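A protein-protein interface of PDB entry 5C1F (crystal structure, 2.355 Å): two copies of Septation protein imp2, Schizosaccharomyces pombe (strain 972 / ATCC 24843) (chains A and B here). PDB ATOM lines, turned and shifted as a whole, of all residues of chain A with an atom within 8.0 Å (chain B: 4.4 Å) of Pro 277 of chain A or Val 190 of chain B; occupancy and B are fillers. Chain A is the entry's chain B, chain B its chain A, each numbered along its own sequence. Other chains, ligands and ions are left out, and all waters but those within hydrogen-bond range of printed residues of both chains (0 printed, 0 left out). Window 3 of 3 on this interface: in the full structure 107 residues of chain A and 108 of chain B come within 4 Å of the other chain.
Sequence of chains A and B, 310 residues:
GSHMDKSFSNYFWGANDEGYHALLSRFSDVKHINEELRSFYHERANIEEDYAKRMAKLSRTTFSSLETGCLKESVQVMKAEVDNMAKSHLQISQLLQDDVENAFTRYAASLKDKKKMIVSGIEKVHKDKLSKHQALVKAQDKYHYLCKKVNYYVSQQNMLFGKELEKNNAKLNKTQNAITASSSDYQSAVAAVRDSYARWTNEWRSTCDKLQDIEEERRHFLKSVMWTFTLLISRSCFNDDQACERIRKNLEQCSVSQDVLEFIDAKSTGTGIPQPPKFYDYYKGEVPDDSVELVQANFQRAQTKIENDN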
ATOM      1  N   PRO A 274      -2.507   5.136   3.663  1.00  0.00           N
ATOM      2  CA  PRO A 274      -3.378   6.262   3.306  1.00  0.00           C
ATOM      3  C   PRO A 274      -4.332   5.906   2.171  1.00  0.00           C
ATOM      4  O   PRO A 274      -3.887   5.451   1.118  1.00  0.00           O
ATOM      5  CB  PRO A 274      -2.389   7.351   2.870  1.00  0.00           C
ATOM      6  CG  PRO A 274      -1.081   6.955   3.489  1.00  0.00           C
ATOM      7  CD  PRO A 274      -1.082   5.461   3.483  1.00  0.00           C
ATOM      8  N   GLN A 275      -5.627   6.107   2.390  1.00  0.00           N
ATOM      9  CA  GLN A 275      -6.630   5.793   1.380  1.00  0.00           C
ATOM     10  C   GLN A 275      -6.916   7.009   0.506  1.00  0.00           C
ATOM     11  O   GLN A 275      -6.802   8.144   0.968  1.00  0.00           O
ATOM     12  CB  GLN A 275      -7.917   5.291   2.043  1.00  0.00           C
ATOM     13  CG  GLN A 275      -7.753   3.975   2.789  1.00  0.00           C
ATOM     14  CD  GLN A 275      -7.163   2.879   1.920  1.00  0.00           C
ATOM     15  OE1 GLN A 275      -6.159   2.262   2.280  1.00  0.00           O
ATOM     16  NE2 GLN A 275      -7.788   2.627   0.774  1.00  0.00           N
ATOM     17  N   PRO A 276      -7.280   6.777  -0.769  1.00  0.00           N
ATOM     18  CA  PRO A 276      -7.575   7.865  -1.711  1.00  0.00           C
ATOM     19  C   PRO A 276      -8.785   8.707  -1.303  1.00  0.00           C
ATOM     20  O   PRO A 276      -9.739   8.179  -0.730  1.00  0.00           O
ATOM     21  CB  PRO A 276      -7.849   7.125  -3.027  1.00  0.00           C
ATOM     22  CG  PRO A 276      -8.235   5.741  -2.615  1.00  0.00           C
ATOM     23  CD  PRO A 276      -7.397   5.454  -1.408  1.00  0.00           C
ATOM     24  N   PRO A 277      -8.742  10.015  -1.592  1.00  0.00           N
ATOM     25  CA  PRO A 277      -9.842  10.935  -1.288  1.00  0.00           C
ATOM     26  C   PRO A 277     -11.085  10.617  -2.110  1.00  0.00           C
ATOM     27  O   PRO A 277     -10.965  10.317  -3.299  1.00  0.00           O
ATOM     28  CB  PRO A 277      -9.274  12.306  -1.666  1.00  0.00           C
ATOM     29  CG  PRO A 277      -7.788  12.118  -1.717  1.00  0.00           C
ATOM     30  CD  PRO A 277      -7.592  10.714  -2.190  1.00  0.00           C
ATOM     31  N   LYS A 278     -12.257  10.694  -1.488  1.00  0.00           N
ATOM     32  CA  LYS A 278     -13.499  10.333  -2.162  1.00  0.00           C
ATOM     33  C   LYS A 278     -14.201  11.541  -2.780  1.00  0.00           C
ATOM     34  O   LYS A 278     -13.831  12.687  -2.531  1.00  0.00           O
ATOM     35  CB  LYS A 278     -14.440   9.620  -1.187  1.00  0.00           C
ATOM     36  CG  LYS A 278     -14.295   8.100  -1.177  1.00  0.00           C
ATOM     37  CD  LYS A 278     -14.966   7.480   0.045  1.00  0.00           C
ATOM     38  CE  LYS A 278     -15.111   5.968  -0.092  1.00  0.00           C
ATOM     39  NZ  LYS A 278     -16.177   5.598  -1.069  1.00  0.00           N
ATOM     40  N   PHE A 279     -15.208  11.262  -3.600  1.00  0.00           N
ATOM     41  CA  PHE A 279     -16.007  12.297  -4.238  1.00  0.00           C
ATOM     42  C   PHE A 279     -17.032  12.850  -3.259  1.00  0.00           C
ATOM     43  O   PHE A 279     -17.897  12.118  -2.779  1.00  0.00           O
ATOM     44  CB  PHE A 279     -16.701  11.735  -5.483  1.00  0.00           C
ATOM     45  CG  PHE A 279     -17.603  12.715  -6.183  1.00  0.00           C
ATOM     46  CD1 PHE A 279     -17.105  13.554  -7.167  1.00  0.00           C
ATOM     47  CD2 PHE A 279     -18.955  12.778  -5.878  1.00  0.00           C
ATOM     48  CE1 PHE A 279     -17.933  14.446  -7.820  1.00  0.00           C
ATOM     49  CE2 PHE A 279     -19.787  13.671  -6.527  1.00  0.00           C
ATOM     50  CZ  PHE A 279     -19.276  14.507  -7.499  1.00  0.00           C
ATOM     51  N   TYR A 280     -16.935  14.141  -2.962  1.00  0.00           N
ATOM     52  CA  TYR A 280     -17.897  14.784  -2.077  1.00  0.00           C
ATOM     53  C   TYR A 280     -18.870  15.632  -2.882  1.00  0.00           C
ATOM     54  O   TYR A 280     -18.502  16.676  -3.417  1.00  0.00           O
ATOM     55  CB  TYR A 280     -17.186  15.636  -1.026  1.00  0.00           C
ATOM     56  CG  TYR A 280     -16.287  14.836  -0.109  1.00  0.00           C
ATOM     57  CD1 TYR A 280     -16.804  14.157   0.984  1.00  0.00           C
ATOM     58  CD2 TYR A 280     -14.922  14.755  -0.344  1.00  0.00           C
ATOM     59  CE1 TYR A 280     -15.983  13.419   1.824  1.00  0.00           C
ATOM     60  CE2 TYR A 280     -14.093  14.021   0.487  1.00  0.00           C
ATOM     61  CZ  TYR A 280     -14.628  13.355   1.569  1.00  0.00           C
ATOM     62  OH  TYR A 280     -13.804  12.623   2.398  1.00  0.00           O
ATOM     63  N   ASP A 289     -14.927  15.052   4.684  1.00  0.00           N
ATOM     64  CA  ASP A 289     -14.321  14.588   5.917  1.00  0.00           C
ATOM     65  C   ASP A 289     -12.832  14.488   5.629  1.00  0.00           C
ATOM     66  O   ASP A 289     -12.355  13.467   5.150  1.00  0.00           O
ATOM     67  CB  ASP A 289     -14.904  13.243   6.362  1.00  0.00           C
ATOM     68  CG  ASP A 289     -14.626  12.939   7.822  1.00  0.00           C
ATOM     69  OD1 ASP A 289     -13.704  13.559   8.398  1.00  0.00           O
ATOM     70  OD2 ASP A 289     -15.331  12.084   8.397  1.00  0.00           O
ATOM     71  N   SER A 291     -10.362  13.679   6.857  1.00  0.00           N
ATOM     72  CA  SER A 291      -9.600  12.624   7.505  1.00  0.00           C
ATOM     73  C   SER A 291      -9.015  11.685   6.457  1.00  0.00           C
ATOM     74  O   SER A 291      -9.665  11.379   5.456  1.00  0.00           O
ATOM     75  CB  SER A 291     -10.490  11.855   8.483  1.00  0.00           C
ATOM     76  OG  SER A 291      -9.732  10.978   9.291  1.00  0.00           O
ATOM     77  N   VAL A 292      -7.785  11.240   6.686  1.00  0.00           N
ATOM     78  CA  VAL A 292      -7.176  10.231   5.831  1.00  0.00           C
ATOM     79  C   VAL A 292      -7.502   8.856   6.396  1.00  0.00           C
ATOM     80  O   VAL A 292      -6.979   8.478   7.445  1.00  0.00           O
ATOM     81  CB  VAL A 292      -5.644  10.400   5.731  1.00  0.00           C
ATOM     82  CG1 VAL A 292      -5.068   9.431   4.710  1.00  0.00           C
ATOM     83  CG2 VAL A 292      -5.283  11.837   5.376  1.00  0.00           C
ATOM     84  N   GLU A 293      -8.382   8.119   5.722  1.00  0.00           N
ATOM     85  CA  GLU A 293      -8.716   6.772   6.168  1.00  0.00           C
ATOM     86  C   GLU A 293      -7.475   5.894   6.090  1.00  0.00           C
ATOM     87  O   GLU A 293      -6.754   5.908   5.092  1.00  0.00           O
ATOM     88  CB  GLU A 293      -9.849   6.163   5.334  1.00  0.00           C
ATOM     89  CG  GLU A 293     -10.298   4.789   5.835  1.00  0.00           C
ATOM     90  CD  GLU A 293     -11.348   4.136   4.951  1.00  0.00           C
ATOM     91  OE1 GLU A 293     -11.919   4.828   4.081  1.00  0.00           O
ATOM     92  OE2 GLU A 293     -11.601   2.924   5.128  1.00  0.00           O
ATOM     93  N   HIS B 133      -3.056  13.893  -7.154  1.00  0.00           N
ATOM     94  CA  HIS B 133      -3.652  14.468  -5.950  1.00  0.00           C
ATOM     95  C   HIS B 133      -3.820  15.979  -6.076  1.00  0.00           C
ATOM     96  O   HIS B 133      -4.832  16.533  -5.641  1.00  0.00           O
ATOM     97  CB  HIS B 133      -2.811  14.135  -4.714  1.00  0.00           C
ATOM     98  CG  HIS B 133      -3.510  14.417  -3.419  1.00  0.00           C
ATOM     99  ND1 HIS B 133      -3.500  15.658  -2.820  1.00  0.00           N
ATOM    100  CD2 HIS B 133      -4.256  13.620  -2.618  1.00  0.00           C
ATOM    101  CE1 HIS B 133      -4.202  15.612  -1.701  1.00  0.00           C
ATOM    102  NE2 HIS B 133      -4.671  14.387  -1.556  1.00  0.00           N
ATOM    103  N   LEU B 136      -6.670  16.539  -8.296  1.00  0.00           N
ATOM    104  CA  LEU B 136      -7.906  16.263  -7.578  1.00  0.00           C
ATOM    105  C   LEU B 136      -8.353  17.471  -6.765  1.00  0.00           C
ATOM    106  O   LEU B 136      -9.528  17.835  -6.776  1.00  0.00           O
ATOM    107  CB  LEU B 136      -7.737  15.051  -6.665  1.00  0.00           C
ATOM    108  CG  LEU B 136      -8.937  14.736  -5.773  1.00  0.00           C
ATOM    109  CD1 LEU B 136     -10.189  14.576  -6.609  1.00  0.00           C
ATOM    110  CD2 LEU B 136      -8.674  13.482  -4.969  1.00  0.00           C
ATOM    111  N   TYR B 186     -14.225  16.505 -11.846  1.00  0.00           N
ATOM    112  CA  TYR B 186     -13.931  16.187 -10.451  1.00  0.00           C
ATOM    113  C   TYR B 186     -13.965  14.672 -10.239  1.00  0.00           C
ATOM    114  O   TYR B 186     -13.021  14.094  -9.699  1.00  0.00           O
ATOM    115  CB  TYR B 186     -14.930  16.903  -9.534  1.00  0.00           C
ATOM    116  CG  TYR B 186     -14.792  16.653  -8.041  1.00  0.00           C
ATOM    117  CD1 TYR B 186     -13.630  16.125  -7.489  1.00  0.00           C
ATOM    118  CD2 TYR B 186     -15.840  16.950  -7.185  1.00  0.00           C
ATOM    119  CE1 TYR B 186     -13.528  15.896  -6.126  1.00  0.00           C
ATOM    120  CE2 TYR B 186     -15.746  16.728  -5.827  1.00  0.00           C
ATOM    121  CZ  TYR B 186     -14.591  16.202  -5.302  1.00  0.00           C
ATOM    122  OH  TYR B 186     -14.506  15.986  -3.947  1.00  0.00           O
ATOM    123  N   GLN B 187     -15.040  14.028 -10.680  1.00  0.00           N
ATOM    124  CA  GLN B 187     -15.181  12.586 -10.508  1.00  0.00           C
ATOM    125  C   GLN B 187     -14.100  11.826 -11.273  1.00  0.00           C
ATOM    126  O   GLN B 187     -13.665  10.756 -10.848  1.00  0.00           O
ATOM    127  CB  GLN B 187     -16.567  12.121 -10.955  1.00  0.00           C
ATOM    128  CG  GLN B 187     -16.964  10.763 -10.396  1.00  0.00           C
ATOM    129  CD  GLN B 187     -18.326  10.788  -9.730  1.00  0.00           C
ATOM    130  OE1 GLN B 187     -19.163  11.640 -10.036  1.00  0.00           O
ATOM    131  NE2 GLN B 187     -18.552   9.861  -8.806  1.00  0.00           N
ATOM    132  N   SER B 188     -13.673  12.381 -12.403  1.00  0.00           N
ATOM    133  CA  SER B 188     -12.564  11.807 -13.154  1.00  0.00           C
ATOM    134  C   SER B 188     -11.288  11.901 -12.332  1.00  0.00           C
ATOM    135  O   SER B 188     -10.479  10.974 -12.314  1.00  0.00           O
ATOM    136  CB  SER B 188     -12.383  12.518 -14.495  1.00  0.00           C
ATOM    137  OG  SER B 188     -13.512  12.330 -15.327  1.00  0.00           O
ATOM    138  N   ALA B 189     -11.122  13.030 -11.647  1.00  0.00           N
ATOM    139  CA  ALA B 189      -9.954  13.259 -10.807  1.00  0.00           C
ATOM    140  C   ALA B 189      -9.944  12.291  -9.633  1.00  0.00           C
ATOM    141  O   ALA B 189      -8.894  11.776  -9.258  1.00  0.00           O
ATOM    142  CB  ALA B 189      -9.921  14.697 -10.314  1.00  0.00           C
ATOM    143  N   VAL B 190     -11.118  12.049  -9.058  1.00  0.00           N
ATOM    144  CA  VAL B 190     -11.263  11.065  -7.990  1.00  0.00           C
ATOM    145  C   VAL B 190     -10.860   9.671  -8.478  1.00  0.00           C
ATOM    146  O   VAL B 190     -10.126   8.953  -7.798  1.00  0.00           O
ATOM    147  CB  VAL B 190     -12.711  11.026  -7.451  1.00  0.00           C
ATOM    148  CG1 VAL B 190     -12.884   9.890  -6.453  1.00  0.00           C
ATOM    149  CG2 VAL B 190     -13.081  12.358  -6.822  1.00  0.00           C
ATOM    150  N   ALA B 191     -11.333   9.302  -9.664  1.00  0.00           N
ATOM    151  CA  ALA B 191     -11.035   7.991 -10.229  1.00  0.00           C
ATOM    152  C   ALA B 191      -9.539   7.817 -10.485  1.00  0.00           C
ATOM    153  O   ALA B 191      -8.959   6.782 -10.150  1.00  0.00           O
ATOM    154  CB  ALA B 191     -11.818   7.779 -11.516  1.00  0.00           C
ATOM    155  N   ALA B 192      -8.921   8.836 -11.073  1.00  0.00           N
ATOM    156  CA  ALA B 192      -7.507   8.775 -11.429  1.00  0.00           C
ATOM    157  C   ALA B 192      -6.598   8.710 -10.198  1.00  0.00           C
ATOM    158  O   ALA B 192      -5.584   8.012 -10.207  1.00  0.00           O
ATOM    159  CB  ALA B 192      -7.138   9.966 -12.298  1.00  0.00           C
ATOM    160  N   VAL B 193      -6.963   9.433  -9.144  1.00  0.00           N
ATOM    161  CA  VAL B 193      -6.195   9.410  -7.902  1.00  0.00           C
ATOM    162  C   VAL B 193      -6.321   8.055  -7.206  1.00  0.00           C
ATOM    163  O   VAL B 193      -5.380   7.584  -6.571  1.00  0.00           O
ATOM    164  CB  VAL B 193      -6.639  10.539  -6.940  1.00  0.00           C
ATOM    165  CG1 VAL B 193      -5.970  10.400  -5.581  1.00  0.00           C
ATOM    166  CG2 VAL B 193      -6.309  11.894  -7.536  1.00  0.00           C
ATOM    167  N   ARG B 194      -7.493   7.441  -7.314  1.00  0.00           N
ATOM    168  CA  ARG B 194      -7.709   6.129  -6.724  1.00  0.00           C
ATOM    169  C   ARG B 194      -6.778   5.107  -7.358  1.00  0.00           C
ATOM    170  O   ARG B 194      -6.159   4.303  -6.660  1.00  0.00           O
ATOM    171  CB  ARG B 194      -9.169   5.686  -6.887  1.00  0.00           C
ATOM    172  CG  ARG B 194      -9.371   4.165  -6.741  1.00  0.00           C
ATOM    173  CD  ARG B 194     -10.817   3.741  -6.667  1.00  0.00           C
ATOM    174  NE  ARG B 194     -11.678   4.349  -7.673  1.00  0.00           N
ATOM    175  CZ  ARG B 194     -11.645   4.057  -8.972  1.00  0.00           C
ATOM    176  NH1 ARG B 194     -10.773   3.178  -9.454  1.00  0.00           N
ATOM    177  NH2 ARG B 194     -12.469   4.668  -9.814  1.00  0.00           N
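No position is printed for both chains. Of the 10 pairs that touch across the chains among the printed residues, none has its exchanged pair printed and touching as well.
Of the printed residues of chain B, Pro 276 of chain A touches Arg 194 (3.8 Å). Pro 277 of chain A touches four residues of chain B. Of the printed residues of chain B, Lys 278 of chain A touches Tyr 186 (3.7 Å). Of the printed residues of chain B, Phe 279 of chain A touches Tyr 186, Gln 187 and Val 190. Of the printed residues of chain A, Leu 136 of chain B touches Pro 277 (3.6 Å). Of the printed residues of chain A, Tyr 186 of chain B touches Lys 278, Phe 279 and Tyr 280. No residue of chain A comes within 4 Å of Ala 189 of chain B. Val 190 of chain B touches just these residues of chain A: Pro 277 (3.7 Å) and Phe 279 (3.9 Å). No residue of chain A comes within 4 Å of Ala 191 of chain B. The nearest printed residue of chain B that does not touch Pro 277 of chain A is Arg 194 of chain B (6.0 Å).
Hydrophobic or aromatic side chains of chain A that line the printed part of chain B: Pro 276, Pro 277, Phe 279 and Tyr 280. Hydrophobic or aromatic side chains of chain B within 4 Å of the printed part of chain A: His 133, Leu 136, Tyr 186, Val 190 and Val 193. Among the printed residues, 10 pairs touch across the chains. Among the printed residues, no Asp or Glu carboxylate lies within 4 Å of a Lys or Arg side-chain nitrogen of the other chain.
Pro 276 of chain A touches Arg 194 of chain B. CG of Pro 277 of chain A touches NE2 of His 133 of chain B, at 3.9 Å. Leu 136 of chain B touches Pro 277 of chain A. CG1 of Val 190 of chain B touches O of Pro 277 of chain A (3.7 Å). Pro 277 of chain A touches Val 193 of chain B. Lys 278 of chain A touches Tyr 186 of chain B (O to OH, 3.7 Å). Phe 279 of chain A touches Tyr 186 of chain B. Phe 279 of chain A touches Gln 187 of chain B (CE1 to OE1, 3.8 Å). CG2 of Val 190 of chain B touches CA of Phe 279 of chain A (3.9 Å).
OH of Tyr 280 of chain A is in hydrogen-bond range of O of Asp 289 of chain A (3.2 Å).
The backbone NH (N) of Tyr 280 of chain A sits at hydrogen-bond distance from the side-chain hydroxyl (OH) of Tyr 186 of chain B (3.2 Å).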
